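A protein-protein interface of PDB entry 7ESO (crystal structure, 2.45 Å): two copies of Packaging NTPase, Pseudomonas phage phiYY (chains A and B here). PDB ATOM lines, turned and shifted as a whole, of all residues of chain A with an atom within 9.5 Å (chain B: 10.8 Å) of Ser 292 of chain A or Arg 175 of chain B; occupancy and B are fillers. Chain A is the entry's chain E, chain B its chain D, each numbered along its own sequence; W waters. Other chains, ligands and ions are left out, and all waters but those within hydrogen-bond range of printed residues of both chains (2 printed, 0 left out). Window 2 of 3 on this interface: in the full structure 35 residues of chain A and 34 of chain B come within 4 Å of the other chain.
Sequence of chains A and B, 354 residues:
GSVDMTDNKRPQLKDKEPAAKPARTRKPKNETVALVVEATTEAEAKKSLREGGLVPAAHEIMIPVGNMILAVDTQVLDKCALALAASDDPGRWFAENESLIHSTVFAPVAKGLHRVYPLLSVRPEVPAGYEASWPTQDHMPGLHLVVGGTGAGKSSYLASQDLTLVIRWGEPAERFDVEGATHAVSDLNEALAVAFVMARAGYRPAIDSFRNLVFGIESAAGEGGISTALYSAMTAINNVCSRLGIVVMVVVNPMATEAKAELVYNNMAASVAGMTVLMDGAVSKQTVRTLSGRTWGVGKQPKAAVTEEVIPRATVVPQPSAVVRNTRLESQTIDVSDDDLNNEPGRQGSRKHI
The guanidinium group of Arg 289 of chain A lies within salt-bridge range of the side-chain carboxylate of Glu 174 of chain B (3.4 Å). NH2 of Arg 175 of chain B lies within hydrogen-bond range of O of Ser 292 of chain A (2.8 Å).
The side-chain carboxylate of Glu 174 of chain B is in salt-bridge range of the guanidinium group of Arg 168 of chain B, 3.8 Å away. NE of Arg 168 of chain B lies within salt-bridge range of OD1 of Asp 177 of chain B (2.6 Å). The backbone carbonyl oxygen (O) of Asp 138 of chain A lies within hydrogen-bond range of the backbone NH (N) of Leu 291 of chain A, at 2.9 Å. The backbone carbonyl oxygen (O) of Ala 273 of chain A lies within hydrogen-bond range of the backbone NH (N) of Arg 289 of chain A, at 2.7 Å.
CG of Pro 124 of chain A touches O of Glu 171 of chain B, at 3.5 Å. Ala 173 of chain B touches Pro 124 of chain A. O of Pro 124 of chain A touches CB of Ala 184 of chain B (3.5 Å). Glu 174 of chain B touches Met 140 of chain A (O to CE, 3.8 Å). Pro 172 of chain B touches Arg 289 of chain A (CG to NH1, 3.6 Å). O of Ala 173 of chain B touches CD of Arg 289 of chain A (3.9 Å). Arg 175 of chain B touches Leu 291 of chain A. Glu 179 of chain B touches Leu 291 of chain A.
Of chain A, only Leu 291 (3.9 Å) and Ser 292 (2.8 Å) come within 4 Å of Arg 175 of chain B. Thr 290 of chain A touches none of the printed residues of chain B. Of chain B, only Arg 175 (3.9 Å) and Glu 179 (3.9 Å) come within 4 Å of Leu 291 of chain A. No residue of chain B comes within 4 Å of Gly 293 of chain A. Val 178 of chain B touches one residue of chain A. Of the printed residues of chain B, Arg 289 of chain A touches Pro 172 (3.6 Å), Ala 173 (3.9 Å) and Glu 174 (3.4 Å). Of the printed residues of chain A, Pro 172 of chain B touches Arg 289. Val 288 of chain A touches none of the printed residues of chain B. Asp 208 of chain B touches none of the printed residues of chain A. The nearest residue of chain B that does not touch Ser 292 of chain A is Glu 179 of chain B (5.6 Å). The nearest printed residue of chain A that does not touch Arg 175 of chain B is Met 140 of chain A (4.1 Å). The nearest printed residue of chain B that does not touch Arg 289 of chain A is Arg 175 of chain B (5.8 Å).
Hydrophobic or aromatic side chains of chain B within 4 Å of the printed part of chain A: Pro 172, Ala 173, Val 178 and Ala 184. Of the 19 printed residues of chain A, 7 touch a printed residue of chain B. Printed residues of chain A that touch a printed residue of chain B: Pro 124, Val 126, Met 140, Ser 242, Arg 289, Leu 291 and Ser 292. Hydrophobic or aromatic side chains of chain A within 4 Å of the printed part of chain B: Pro 124, Val 126 and Met 140. Among the printed residues, Asp or Glu carboxylates within 4 Å of a Lys or Arg side-chain nitrogen of the other chain: Arg 289 of chain A with Glu 174 of chain B.
No position is printed for both chains.
Water W1 bridges O of Ala 173 of chain B (2.5 Å) and O of Pro 141 of chain A (3.1 Å). Water W2 bridges N of Arg 175 of chain B and O of Thr 290 of chain A.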
ATOM      1  N   PRO A 124     -20.993   5.707  17.384  1.00  0.00           N
ATOM      2  CA  PRO A 124     -21.284   7.137  17.202  1.00  0.00           C
ATOM      3  C   PRO A 124     -20.063   7.906  16.725  1.00  0.00           C
ATOM      4  O   PRO A 124     -19.074   8.034  17.453  1.00  0.00           O
ATOM      5  CB  PRO A 124     -21.718   7.597  18.604  1.00  0.00           C
ATOM      6  CG  PRO A 124     -21.750   6.359  19.465  1.00  0.00           C
ATOM      7  CD  PRO A 124     -20.868   5.357  18.809  1.00  0.00           C
ATOM      8  N   GLU A 125     -20.113   8.407  15.497  1.00  0.00           N
ATOM      9  CA  GLU A 125     -19.055   9.233  14.944  1.00  0.00           C
ATOM     10  C   GLU A 125     -19.666  10.405  14.205  1.00  0.00           C
ATOM     11  O   GLU A 125     -20.816  10.355  13.766  1.00  0.00           O
ATOM     12  CB  GLU A 125     -18.144   8.463  13.985  1.00  0.00           C
ATOM     13  CG  GLU A 125     -16.952   7.798  14.636  1.00  0.00           C
ATOM     14  CD  GLU A 125     -16.123   7.010  13.636  1.00  0.00           C
ATOM     15  OE1 GLU A 125     -16.436   7.065  12.423  1.00  0.00           O
ATOM     16  OE2 GLU A 125     -15.151   6.354  14.063  1.00  0.00           O
ATOM     17  N   VAL A 126     -18.882  11.471  14.079  1.00  0.00           N
ATOM     18  CA  VAL A 126     -19.262  12.632  13.279  1.00  0.00           C
ATOM     19  C   VAL A 126     -18.089  12.979  12.374  1.00  0.00           C
ATOM     20  O   VAL A 126     -16.975  13.194  12.872  1.00  0.00           O
ATOM     21  CB  VAL A 126     -19.647  13.830  14.156  1.00  0.00           C
ATOM     22  CG1 VAL A 126     -20.233  14.938  13.295  1.00  0.00           C
ATOM     23  CG2 VAL A 126     -20.637  13.406  15.217  1.00  0.00           C
ATOM     24  N   TYR A 130     -18.546  18.552   9.584  1.00  0.00           N
ATOM     25  CA  TYR A 130     -19.974  18.406   9.340  1.00  0.00           C
ATOM     26  C   TYR A 130     -20.711  19.688   9.727  1.00  0.00           C
ATOM     27  O   TYR A 130     -20.395  20.323  10.736  1.00  0.00           O
ATOM     28  CB  TYR A 130     -20.522  17.217  10.130  1.00  0.00           C
ATOM     29  CG  TYR A 130     -22.029  17.190  10.232  1.00  0.00           C
ATOM     30  CD1 TYR A 130     -22.801  16.634   9.220  1.00  0.00           C
ATOM     31  CD2 TYR A 130     -22.680  17.717  11.341  1.00  0.00           C
ATOM     32  CE1 TYR A 130     -24.173  16.612   9.303  1.00  0.00           C
ATOM     33  CE2 TYR A 130     -24.054  17.703  11.432  1.00  0.00           C
ATOM     34  CZ  TYR A 130     -24.796  17.144  10.417  1.00  0.00           C
ATOM     35  OH  TYR A 130     -26.169  17.119  10.518  1.00  0.00           O
ATOM     36  N   GLN A 137     -31.192  23.915  13.026  1.00  0.00           N
ATOM     37  CA  GLN A 137     -29.830  24.424  13.000  1.00  0.00           C
ATOM     38  C   GLN A 137     -28.936  23.563  13.888  1.00  0.00           C
ATOM     39  O   GLN A 137     -29.312  23.209  15.009  1.00  0.00           O
ATOM     40  CB  GLN A 137     -29.798  25.887  13.442  1.00  0.00           C
ATOM     41  CG  GLN A 137     -28.397  26.481  13.496  1.00  0.00           C
ATOM     42  CD  GLN A 137     -27.695  26.503  12.135  1.00  0.00           C
ATOM     43  OE1 GLN A 137     -28.324  26.713  11.093  1.00  0.00           O
ATOM     44  NE2 GLN A 137     -26.380  26.286  12.146  1.00  0.00           N
ATOM     45  N   ASP A 138     -27.761  23.207  13.364  1.00  0.00           N
ATOM     46  CA  ASP A 138     -26.771  22.381  14.063  1.00  0.00           C
ATOM     47  C   ASP A 138     -27.322  21.005  14.450  1.00  0.00           C
ATOM     48  O   ASP A 138     -26.843  20.387  15.403  1.00  0.00           O
ATOM     49  CB  ASP A 138     -26.217  23.102  15.296  1.00  0.00           C
ATOM     50  CG  ASP A 138     -25.482  24.384  14.940  1.00  0.00           C
ATOM     51  OD1 ASP A 138     -24.992  24.493  13.794  1.00  0.00           O
ATOM     52  OD2 ASP A 138     -25.398  25.284  15.803  1.00  0.00           O
ATOM     53  N   HIS A 139     -28.322  20.519  13.712  1.00  0.00           N
ATOM     54  CA  HIS A 139     -28.882  19.183  13.918  1.00  0.00           C
ATOM     55  C   HIS A 139     -27.792  18.123  13.805  1.00  0.00           C
ATOM     56  O   HIS A 139     -27.123  18.030  12.770  1.00  0.00           O
ATOM     57  CB  HIS A 139     -29.970  18.934  12.868  1.00  0.00           C
ATOM     58  CG  HIS A 139     -30.943  17.853  13.220  1.00  0.00           C
ATOM     59  ND1 HIS A 139     -30.562  16.548  13.453  1.00  0.00           N
ATOM     60  CD2 HIS A 139     -32.295  17.873  13.326  1.00  0.00           C
ATOM     61  CE1 HIS A 139     -31.634  15.818  13.713  1.00  0.00           C
ATOM     62  NE2 HIS A 139     -32.698  16.598  13.641  1.00  0.00           N
ATOM     63  N   MET A 140     -27.611  17.324  14.862  1.00  0.00           N
ATOM     64  CA  MET A 140     -26.655  16.222  14.792  1.00  0.00           C
ATOM     65  C   MET A 140     -27.010  15.304  13.624  1.00  0.00           C
ATOM     66  O   MET A 140     -28.192  15.083  13.342  1.00  0.00           O
ATOM     67  CB  MET A 140     -26.638  15.413  16.091  1.00  0.00           C
ATOM     68  CG  MET A 140     -25.873  16.073  17.237  1.00  0.00           C
ATOM     69  SD  MET A 140     -24.071  16.034  17.073  1.00  0.00           S
ATOM     70  CE  MET A 140     -23.794  14.289  16.760  1.00  0.00           C
ATOM     71  N   PRO A 141     -26.022  14.764  12.922  1.00  0.00           N
ATOM     72  CA  PRO A 141     -26.328  13.797  11.867  1.00  0.00           C
ATOM     73  C   PRO A 141     -26.947  12.537  12.456  1.00  0.00           C
ATOM     74  O   PRO A 141     -26.665  12.144  13.591  1.00  0.00           O
ATOM     75  CB  PRO A 141     -24.960  13.511  11.236  1.00  0.00           C
ATOM     76  CG  PRO A 141     -23.985  13.781  12.326  1.00  0.00           C
ATOM     77  CD  PRO A 141     -24.576  14.881  13.174  1.00  0.00           C
ATOM     78  N   SER A 242     -24.974   9.152  11.100  1.00  0.00           N
ATOM     79  CA  SER A 242     -23.992   9.945  11.832  1.00  0.00           C
ATOM     80  C   SER A 242     -22.589   9.765  11.260  1.00  0.00           C
ATOM     81  O   SER A 242     -21.858  10.746  11.069  1.00  0.00           O
ATOM     82  CB  SER A 242     -24.026   9.567  13.310  1.00  0.00           C
ATOM     83  OG  SER A 242     -23.165  10.393  14.063  1.00  0.00           O
ATOM     84  N   ALA A 273     -31.231  11.153  16.798  1.00  0.00           N
ATOM     85  CA  ALA A 273     -30.742  12.519  16.900  1.00  0.00           C
ATOM     86  C   ALA A 273     -31.891  13.500  17.088  1.00  0.00           C
ATOM     87  O   ALA A 273     -31.786  14.435  17.892  1.00  0.00           O
ATOM     88  CB  ALA A 273     -29.924  12.872  15.659  1.00  0.00           C
ATOM     89  N   VAL A 288     -34.194  17.585  19.595  1.00  0.00           N
ATOM     90  CA  VAL A 288     -33.075  17.465  18.665  1.00  0.00           C
ATOM     91  C   VAL A 288     -31.741  17.582  19.394  1.00  0.00           C
ATOM     92  O   VAL A 288     -31.480  18.576  20.079  1.00  0.00           O
ATOM     93  CB  VAL A 288     -33.151  18.534  17.562  1.00  0.00           C
ATOM     94  CG1 VAL A 288     -31.863  18.531  16.743  1.00  0.00           C
ATOM     95  CG2 VAL A 288     -34.367  18.327  16.675  1.00  0.00           C
ATOM     96  N   ARG A 289     -30.875  16.584  19.227  1.00  0.00           N
ATOM     97  CA  ARG A 289     -29.485  16.706  19.649  1.00  0.00           C
ATOM     98  C   ARG A 289     -28.741  17.589  18.652  1.00  0.00           C
ATOM     99  O   ARG A 289     -28.801  17.356  17.437  1.00  0.00           O
ATOM    100  CB  ARG A 289     -28.824  15.334  19.713  1.00  0.00           C
ATOM    101  CG  ARG A 289     -29.591  14.361  20.558  1.00  0.00           C
ATOM    102  CD  ARG A 289     -28.961  12.982  20.577  1.00  0.00           C
ATOM    103  NE  ARG A 289     -29.960  12.043  21.061  1.00  0.00           N
ATOM    104  CZ  ARG A 289     -30.140  11.730  22.334  1.00  0.00           C
ATOM    105  NH1 ARG A 289     -31.097  10.882  22.669  1.00  0.00           N
ATOM    106  NH2 ARG A 289     -29.353  12.249  23.265  1.00  0.00           N
ATOM    107  N   THR A 290     -28.042  18.601  19.156  1.00  0.00           N
ATOM    108  CA  THR A 290     -27.328  19.525  18.290  1.00  0.00           C
ATOM    109  C   THR A 290     -25.828  19.451  18.544  1.00  0.00           C
ATOM    110  O   THR A 290     -25.350  18.806  19.481  1.00  0.00           O
ATOM    111  CB  THR A 290     -27.806  20.970  18.480  1.00  0.00           C
ATOM    112  OG1 THR A 290     -27.281  21.495  19.706  1.00  0.00           O
ATOM    113  CG2 THR A 290     -29.323  21.029  18.509  1.00  0.00           C
ATOM    114  N   LEU A 291     -25.083  20.145  17.687  1.00  0.00           N
ATOM    115  CA  LEU A 291     -23.640  20.231  17.841  1.00  0.00           C
ATOM    116  C   LEU A 291     -23.221  21.008  19.084  1.00  0.00           C
ATOM    117  O   LEU A 291     -22.034  21.003  19.423  1.00  0.00           O
ATOM    118  CB  LEU A 291     -23.031  20.865  16.592  1.00  0.00           C
ATOM    119  CG  LEU A 291     -23.245  20.050  15.317  1.00  0.00           C
ATOM    120  CD1 LEU A 291     -23.069  20.934  14.086  1.00  0.00           C
ATOM    121  CD2 LEU A 291     -22.292  18.853  15.289  1.00  0.00           C
ATOM    122  N   SER A 292     -24.155  21.665  19.771  1.00  0.00           N
ATOM    123  CA  SER A 292     -23.864  22.334  21.034  1.00  0.00           C
ATOM    124  C   SER A 292     -24.607  21.709  22.205  1.00  0.00           C
ATOM    125  O   SER A 292     -23.984  21.375  23.221  1.00  0.00           O
ATOM    126  CB  SER A 292     -24.217  23.823  20.931  1.00  0.00           C
ATOM    127  OG  SER A 292     -25.557  23.992  20.515  1.00  0.00           O
ATOM    128  N   GLY A 293     -25.924  21.544  22.096  1.00  0.00           N
ATOM    129  CA  GLY A 293     -26.726  20.963  23.166  1.00  0.00           C
ATOM    130  C   GLY A 293     -27.936  20.238  22.628  1.00  0.00           C
ATOM    131  O   GLY A 293     -27.846  19.509  21.629  1.00  0.00           O
ATOM    132  N   ARG A 294     -29.078  20.433  23.279  1.00  0.00           N
ATOM    133  CA  ARG A 294     -30.276  19.670  22.968  1.00  0.00           C
ATOM    134  C   ARG A 294     -31.459  20.619  23.088  1.00  0.00           C
ATOM    135  O   ARG A 294     -31.568  21.347  24.075  1.00  0.00           O
ATOM    136  CB  ARG A 294     -30.375  18.452  23.903  1.00  0.00           C
ATOM    137  CG  ARG A 294     -31.327  17.328  23.505  1.00  0.00           C
ATOM    138  CD  ARG A 294     -30.726  15.987  23.982  1.00  0.00           C
ATOM    139  NE  ARG A 294     -31.681  14.975  24.448  1.00  0.00           N
ATOM    140  CZ  ARG A 294     -32.515  14.271  23.678  1.00  0.00           C
ATOM    141  NH1 ARG A 294     -33.325  13.374  24.235  1.00  0.00           N
ATOM    142  NH2 ARG A 294     -32.539  14.442  22.360  1.00  0.00           N
ATOM    143  N   THR A 295     -32.303  20.663  22.059  1.00  0.00           N
ATOM    144  CA  THR A 295     -33.405  21.611  21.992  1.00  0.00           C
ATOM    145  C   THR A 295     -34.743  20.893  22.114  1.00  0.00           C
ATOM    146  O   THR A 295     -34.929  19.817  21.537  1.00  0.00           O
ATOM    147  CB  THR A 295     -33.367  22.391  20.680  1.00  0.00           C
ATOM    148  OG1 THR A 295     -33.974  21.610  19.648  1.00  0.00           O
ATOM    149  CG2 THR A 295     -31.936  22.681  20.298  1.00  0.00           C
ATOM    150  N   LYS B 154     -26.951  11.456  34.238  1.00  0.00           N
ATOM    151  CA  LYS B 154     -25.886  10.517  33.896  1.00  0.00           C
ATOM    152  C   LYS B 154     -24.578  11.243  33.601  1.00  0.00           C
ATOM    153  O   LYS B 154     -23.566  11.043  34.283  1.00  0.00           O
ATOM    154  CB  LYS B 154     -26.311   9.669  32.693  1.00  0.00           C
ATOM    155  CG  LYS B 154     -25.212   8.778  32.110  1.00  0.00           C
ATOM    156  CD  LYS B 154     -24.501   9.414  30.898  1.00  0.00           C
ATOM    157  CE  LYS B 154     -25.414   9.529  29.678  1.00  0.00           C
ATOM    158  NZ  LYS B 154     -24.722  10.057  28.465  1.00  0.00           N
ATOM    159  N   SER B 155     -24.583  12.095  32.574  1.00  0.00           N
ATOM    160  CA  SER B 155     -23.342  12.688  32.095  1.00  0.00           C
ATOM    161  C   SER B 155     -22.696  13.568  33.159  1.00  0.00           C
ATOM    162  O   SER B 155     -21.462  13.632  33.250  1.00  0.00           O
ATOM    163  CB  SER B 155     -23.610  13.476  30.809  1.00  0.00           C
ATOM    164  OG  SER B 155     -22.412  13.937  30.213  1.00  0.00           O
ATOM    165  N   VAL B 166     -14.535   7.530  28.386  1.00  0.00           N
ATOM    166  CA  VAL B 166     -15.840   6.898  28.363  1.00  0.00           C
ATOM    167  C   VAL B 166     -15.921   6.111  27.066  1.00  0.00           C
ATOM    168  O   VAL B 166     -15.733   6.675  25.979  1.00  0.00           O
ATOM    169  CB  VAL B 166     -16.965   7.938  28.473  1.00  0.00           C
ATOM    170  CG1 VAL B 166     -18.317   7.309  28.142  1.00  0.00           C
ATOM    171  CG2 VAL B 166     -16.968   8.535  29.863  1.00  0.00           C
ATOM    172  N   ARG B 168     -18.068   4.507  24.367  1.00  0.00           N
ATOM    173  CA  ARG B 168     -19.412   4.805  23.890  1.00  0.00           C
ATOM    174  C   ARG B 168     -19.912   3.675  22.996  1.00  0.00           C
ATOM    175  O   ARG B 168     -19.311   3.381  21.956  1.00  0.00           O
ATOM    176  CB  ARG B 168     -19.438   6.144  23.157  1.00  0.00           C
ATOM    177  CG  ARG B 168     -19.262   7.351  24.088  1.00  0.00           C
ATOM    178  CD  ARG B 168     -20.584   7.753  24.736  1.00  0.00           C
ATOM    179  NE  ARG B 168     -21.485   8.378  23.770  1.00  0.00           N
ATOM    180  CZ  ARG B 168     -22.776   8.604  23.986  1.00  0.00           C
ATOM    181  NH1 ARG B 168     -23.328   8.259  25.140  1.00  0.00           N
ATOM    182  NH2 ARG B 168     -23.516   9.176  23.047  1.00  0.00           N
ATOM    183  N   GLU B 171     -25.398   3.983  21.796  1.00  0.00           N
ATOM    184  CA  GLU B 171     -26.123   5.195  22.105  1.00  0.00           C
ATOM    185  C   GLU B 171     -26.116   6.128  20.898  1.00  0.00           C
ATOM    186  O   GLU B 171     -25.159   6.124  20.117  1.00  0.00           O
ATOM    187  CB  GLU B 171     -25.499   5.902  23.316  1.00  0.00           C
ATOM    188  CG  GLU B 171     -25.712   5.161  24.634  1.00  0.00           C
ATOM    189  CD  GLU B 171     -27.148   5.263  25.130  1.00  0.00           C
ATOM    190  OE1 GLU B 171     -27.841   6.232  24.747  1.00  0.00           O
ATOM    191  OE2 GLU B 171     -27.580   4.375  25.898  1.00  0.00           O
ATOM    192  N   PRO B 172     -27.178   6.919  20.705  1.00  0.00           N
ATOM    193  CA  PRO B 172     -27.197   7.870  19.583  1.00  0.00           C
ATOM    194  C   PRO B 172     -26.058   8.868  19.697  1.00  0.00           C
ATOM    195  O   PRO B 172     -25.764   9.379  20.781  1.00  0.00           O
ATOM    196  CB  PRO B 172     -28.559   8.566  19.725  1.00  0.00           C
ATOM    197  CG  PRO B 172     -28.934   8.387  21.169  1.00  0.00           C
ATOM    198  CD  PRO B 172     -28.395   7.018  21.532  1.00  0.00           C
ATOM    199  N   ALA B 173     -25.412   9.143  18.564  1.00  0.00           N
ATOM    200  CA  ALA B 173     -24.346  10.138  18.531  1.00  0.00           C
ATOM    201  C   ALA B 173     -24.855  11.499  18.993  1.00  0.00           C
ATOM    202  O   ALA B 173     -25.838  12.032  18.466  1.00  0.00           O
ATOM    203  CB  ALA B 173     -23.768  10.247  17.123  1.00  0.00           C
ATOM    204  N   GLU B 174     -24.189  12.054  19.993  1.00  0.00           N
ATOM    205  CA  GLU B 174     -24.454  13.407  20.450  1.00  0.00           C
ATOM    206  C   GLU B 174     -23.131  14.161  20.507  1.00  0.00           C
ATOM    207  O   GLU B 174     -22.085  13.656  20.085  1.00  0.00           O
ATOM    208  CB  GLU B 174     -25.176  13.408  21.803  1.00  0.00           C
ATOM    209  CG  GLU B 174     -24.321  12.958  22.970  1.00  0.00           C
ATOM    210  CD  GLU B 174     -25.151  12.552  24.181  1.00  0.00           C
ATOM    211  OE1 GLU B 174     -24.846  13.019  25.299  1.00  0.00           O
ATOM    212  OE2 GLU B 174     -26.110  11.766  24.019  1.00  0.00           O
ATOM    213  N   ARG B 175     -23.196  15.397  21.007  1.00  0.00           N
ATOM    214  CA  ARG B 175     -22.010  16.237  21.151  1.00  0.00           C
ATOM    215  C   ARG B 175     -20.841  15.548  21.837  1.00  0.00           C
ATOM    216  O   ARG B 175     -19.683  15.699  21.427  1.00  0.00           O
ATOM    217  CB  ARG B 175     -22.352  17.476  21.958  1.00  0.00           C
ATOM    218  CG  ARG B 175     -21.131  18.326  22.117  1.00  0.00           C
ATOM    219  CD  ARG B 175     -21.381  19.512  22.956  1.00  0.00           C
ATOM    220  NE  ARG B 175     -20.167  20.302  23.061  1.00  0.00           N
ATOM    221  CZ  ARG B 175     -20.176  21.621  23.156  1.00  0.00           C
ATOM    222  NH1 ARG B 175     -19.036  22.297  23.237  1.00  0.00           N
ATOM    223  NH2 ARG B 175     -21.336  22.264  23.154  1.00  0.00           N
ATOM    224  N   PHE B 176     -21.134  14.845  22.935  1.00  0.00           N
ATOM    225  CA  PHE B 176     -20.089  14.237  23.751  1.00  0.00           C
ATOM    226  C   PHE B 176     -19.193  13.320  22.929  1.00  0.00           C
ATOM    227  O   PHE B 176     -17.995  13.205  23.211  1.00  0.00           O
ATOM    228  CB  PHE B 176     -20.730  13.476  24.918  1.00  0.00           C
ATOM    229  CG  PHE B 176     -19.741  12.897  25.885  1.00  0.00           C
ATOM    230  CD1 PHE B 176     -18.927  13.729  26.634  1.00  0.00           C
ATOM    231  CD2 PHE B 176     -19.623  11.523  26.052  1.00  0.00           C
ATOM    232  CE1 PHE B 176     -18.008  13.206  27.529  1.00  0.00           C
ATOM    233  CE2 PHE B 176     -18.705  10.992  26.956  1.00  0.00           C
ATOM    234  CZ  PHE B 176     -17.897  11.839  27.691  1.00  0.00           C
ATOM    235  N   ASP B 177     -19.743  12.678  21.895  1.00  0.00           N
ATOM    236  CA  ASP B 177     -18.921  11.864  21.008  1.00  0.00           C
ATOM    237  C   ASP B 177     -18.040  12.702  20.106  1.00  0.00           C
ATOM    238  O   ASP B 177     -17.115  12.166  19.492  1.00  0.00           O
ATOM    239  CB  ASP B 177     -19.801  10.974  20.140  1.00  0.00           C
ATOM    240  CG  ASP B 177     -20.703  10.114  20.955  1.00  0.00           C
ATOM    241  OD1 ASP B 177     -20.172   9.316  21.749  1.00  0.00           O
ATOM    242  OD2 ASP B 177     -21.937  10.252  20.825  1.00  0.00           O
ATOM    243  N   VAL B 178     -18.308  13.997  20.002  1.00  0.00           N
ATOM    244  CA  VAL B 178     -17.655  14.808  18.986  1.00  0.00           C
ATOM    245  C   VAL B 178     -16.396  15.461  19.538  1.00  0.00           C
ATOM    246  O   VAL B 178     -15.356  15.467  18.878  1.00  0.00           O
ATOM    247  CB  VAL B 178     -18.642  15.865  18.451  1.00  0.00           C
ATOM    248  CG1 VAL B 178     -18.004  16.670  17.321  1.00  0.00           C
ATOM    249  CG2 VAL B 178     -19.987  15.247  18.088  1.00  0.00           C
ATOM    250  N   GLU B 179     -16.474  16.004  20.752  1.00  0.00           N
ATOM    251  CA  GLU B 179     -15.381  16.755  21.365  1.00  0.00           C
ATOM    252  C   GLU B 179     -15.219  16.372  22.830  1.00  0.00           C
ATOM    253  O   GLU B 179     -14.956  17.221  23.689  1.00  0.00           O
ATOM    254  CB  GLU B 179     -15.603  18.262  21.228  1.00  0.00           C
ATOM    255  CG  GLU B 179     -16.990  18.721  21.655  1.00  0.00           C
ATOM    256  CD  GLU B 179     -17.386  20.036  21.017  1.00  0.00           C
ATOM    257  OE1 GLU B 179     -16.509  20.703  20.433  1.00  0.00           O
ATOM    258  OE2 GLU B 179     -18.581  20.387  21.076  1.00  0.00           O
ATOM    259  N   GLY B 180     -15.377  15.085  23.136  1.00  0.00           N
ATOM    260  CA  GLY B 180     -15.148  14.566  24.461  1.00  0.00           C
ATOM    261  C   GLY B 180     -13.940  13.644  24.508  1.00  0.00           C
ATOM    262  O   GLY B 180     -13.285  13.363  23.506  1.00  0.00           O
ATOM    263  N   ALA B 181     -13.641  13.186  25.727  1.00  0.00           N
ATOM    264  CA  ALA B 181     -12.636  12.142  25.948  1.00  0.00           C
ATOM    265  C   ALA B 181     -13.343  10.792  25.868  1.00  0.00           C
ATOM    266  O   ALA B 181     -13.670  10.160  26.874  1.00  0.00           O
ATOM    267  CB  ALA B 181     -11.940  12.334  27.289  1.00  0.00           C
ATOM    268  N   THR B 182     -13.601  10.356  24.635  1.00  0.00           N
ATOM    269  CA  THR B 182     -14.410   9.175  24.380  1.00  0.00           C
ATOM    270  C   THR B 182     -13.703   8.238  23.412  1.00  0.00           C
ATOM    271  O   THR B 182     -12.779   8.626  22.693  1.00  0.00           O
ATOM    272  CB  THR B 182     -15.776   9.538  23.787  1.00  0.00           C
ATOM    273  OG1 THR B 182     -15.605   9.887  22.409  1.00  0.00           O
ATOM    274  CG2 THR B 182     -16.393  10.708  24.520  1.00  0.00           C
ATOM    275  N   HIS B 183     -14.180   6.995  23.393  1.00  0.00           N
ATOM    276  CA  HIS B 183     -13.802   6.009  22.386  1.00  0.00           C
ATOM    277  C   HIS B 183     -15.067   5.285  21.944  1.00  0.00           C
ATOM    278  O   HIS B 183     -15.775   4.709  22.778  1.00  0.00           O
ATOM    279  CB  HIS B 183     -12.764   5.024  22.936  1.00  0.00           C
ATOM    280  CG  HIS B 183     -12.428   3.903  21.998  1.00  0.00           C
ATOM    281  ND1 HIS B 183     -11.722   4.091  20.829  1.00  0.00           N
ATOM    282  CD2 HIS B 183     -12.693   2.574  22.067  1.00  0.00           C
ATOM    283  CE1 HIS B 183     -11.568   2.930  20.216  1.00  0.00           C
ATOM    284  NE2 HIS B 183     -12.150   1.993  20.945  1.00  0.00           N
ATOM    285  N   ALA B 184     -15.352   5.326  20.641  1.00  0.00           N
ATOM    286  CA  ALA B 184     -16.578   4.765  20.089  1.00  0.00           C
ATOM    287  C   ALA B 184     -16.334   3.340  19.613  1.00  0.00           C
ATOM    288  O   ALA B 184     -15.345   3.073  18.923  1.00  0.00           O
ATOM    289  CB  ALA B 184     -17.094   5.626  18.935  1.00  0.00           C
ATOM    290  N   ASP B 208     -20.550   3.627  28.395  1.00  0.00           N
ATOM    291  CA  ASP B 208     -21.845   4.274  28.181  1.00  0.00           C
ATOM    292  C   ASP B 208     -22.349   3.835  26.806  1.00  0.00           C
ATOM    293  O   ASP B 208     -21.996   4.446  25.789  1.00  0.00           O
ATOM    294  CB  ASP B 208     -21.711   5.794  28.289  1.00  0.00           C
ATOM    295  CG  ASP B 208     -23.049   6.504  28.280  1.00  0.00           C
ATOM    296  OD1 ASP B 208     -24.070   5.862  28.613  1.00  0.00           O
ATOM    297  OD2 ASP B 208     -23.077   7.710  27.944  1.00  0.00           O
HETATM  298  O   HOH W   1     -27.100  11.183  16.515  1.00  0.00           O
HETATM  299  O   HOH W   2     -25.607  16.698  21.451  1.00  0.00           O
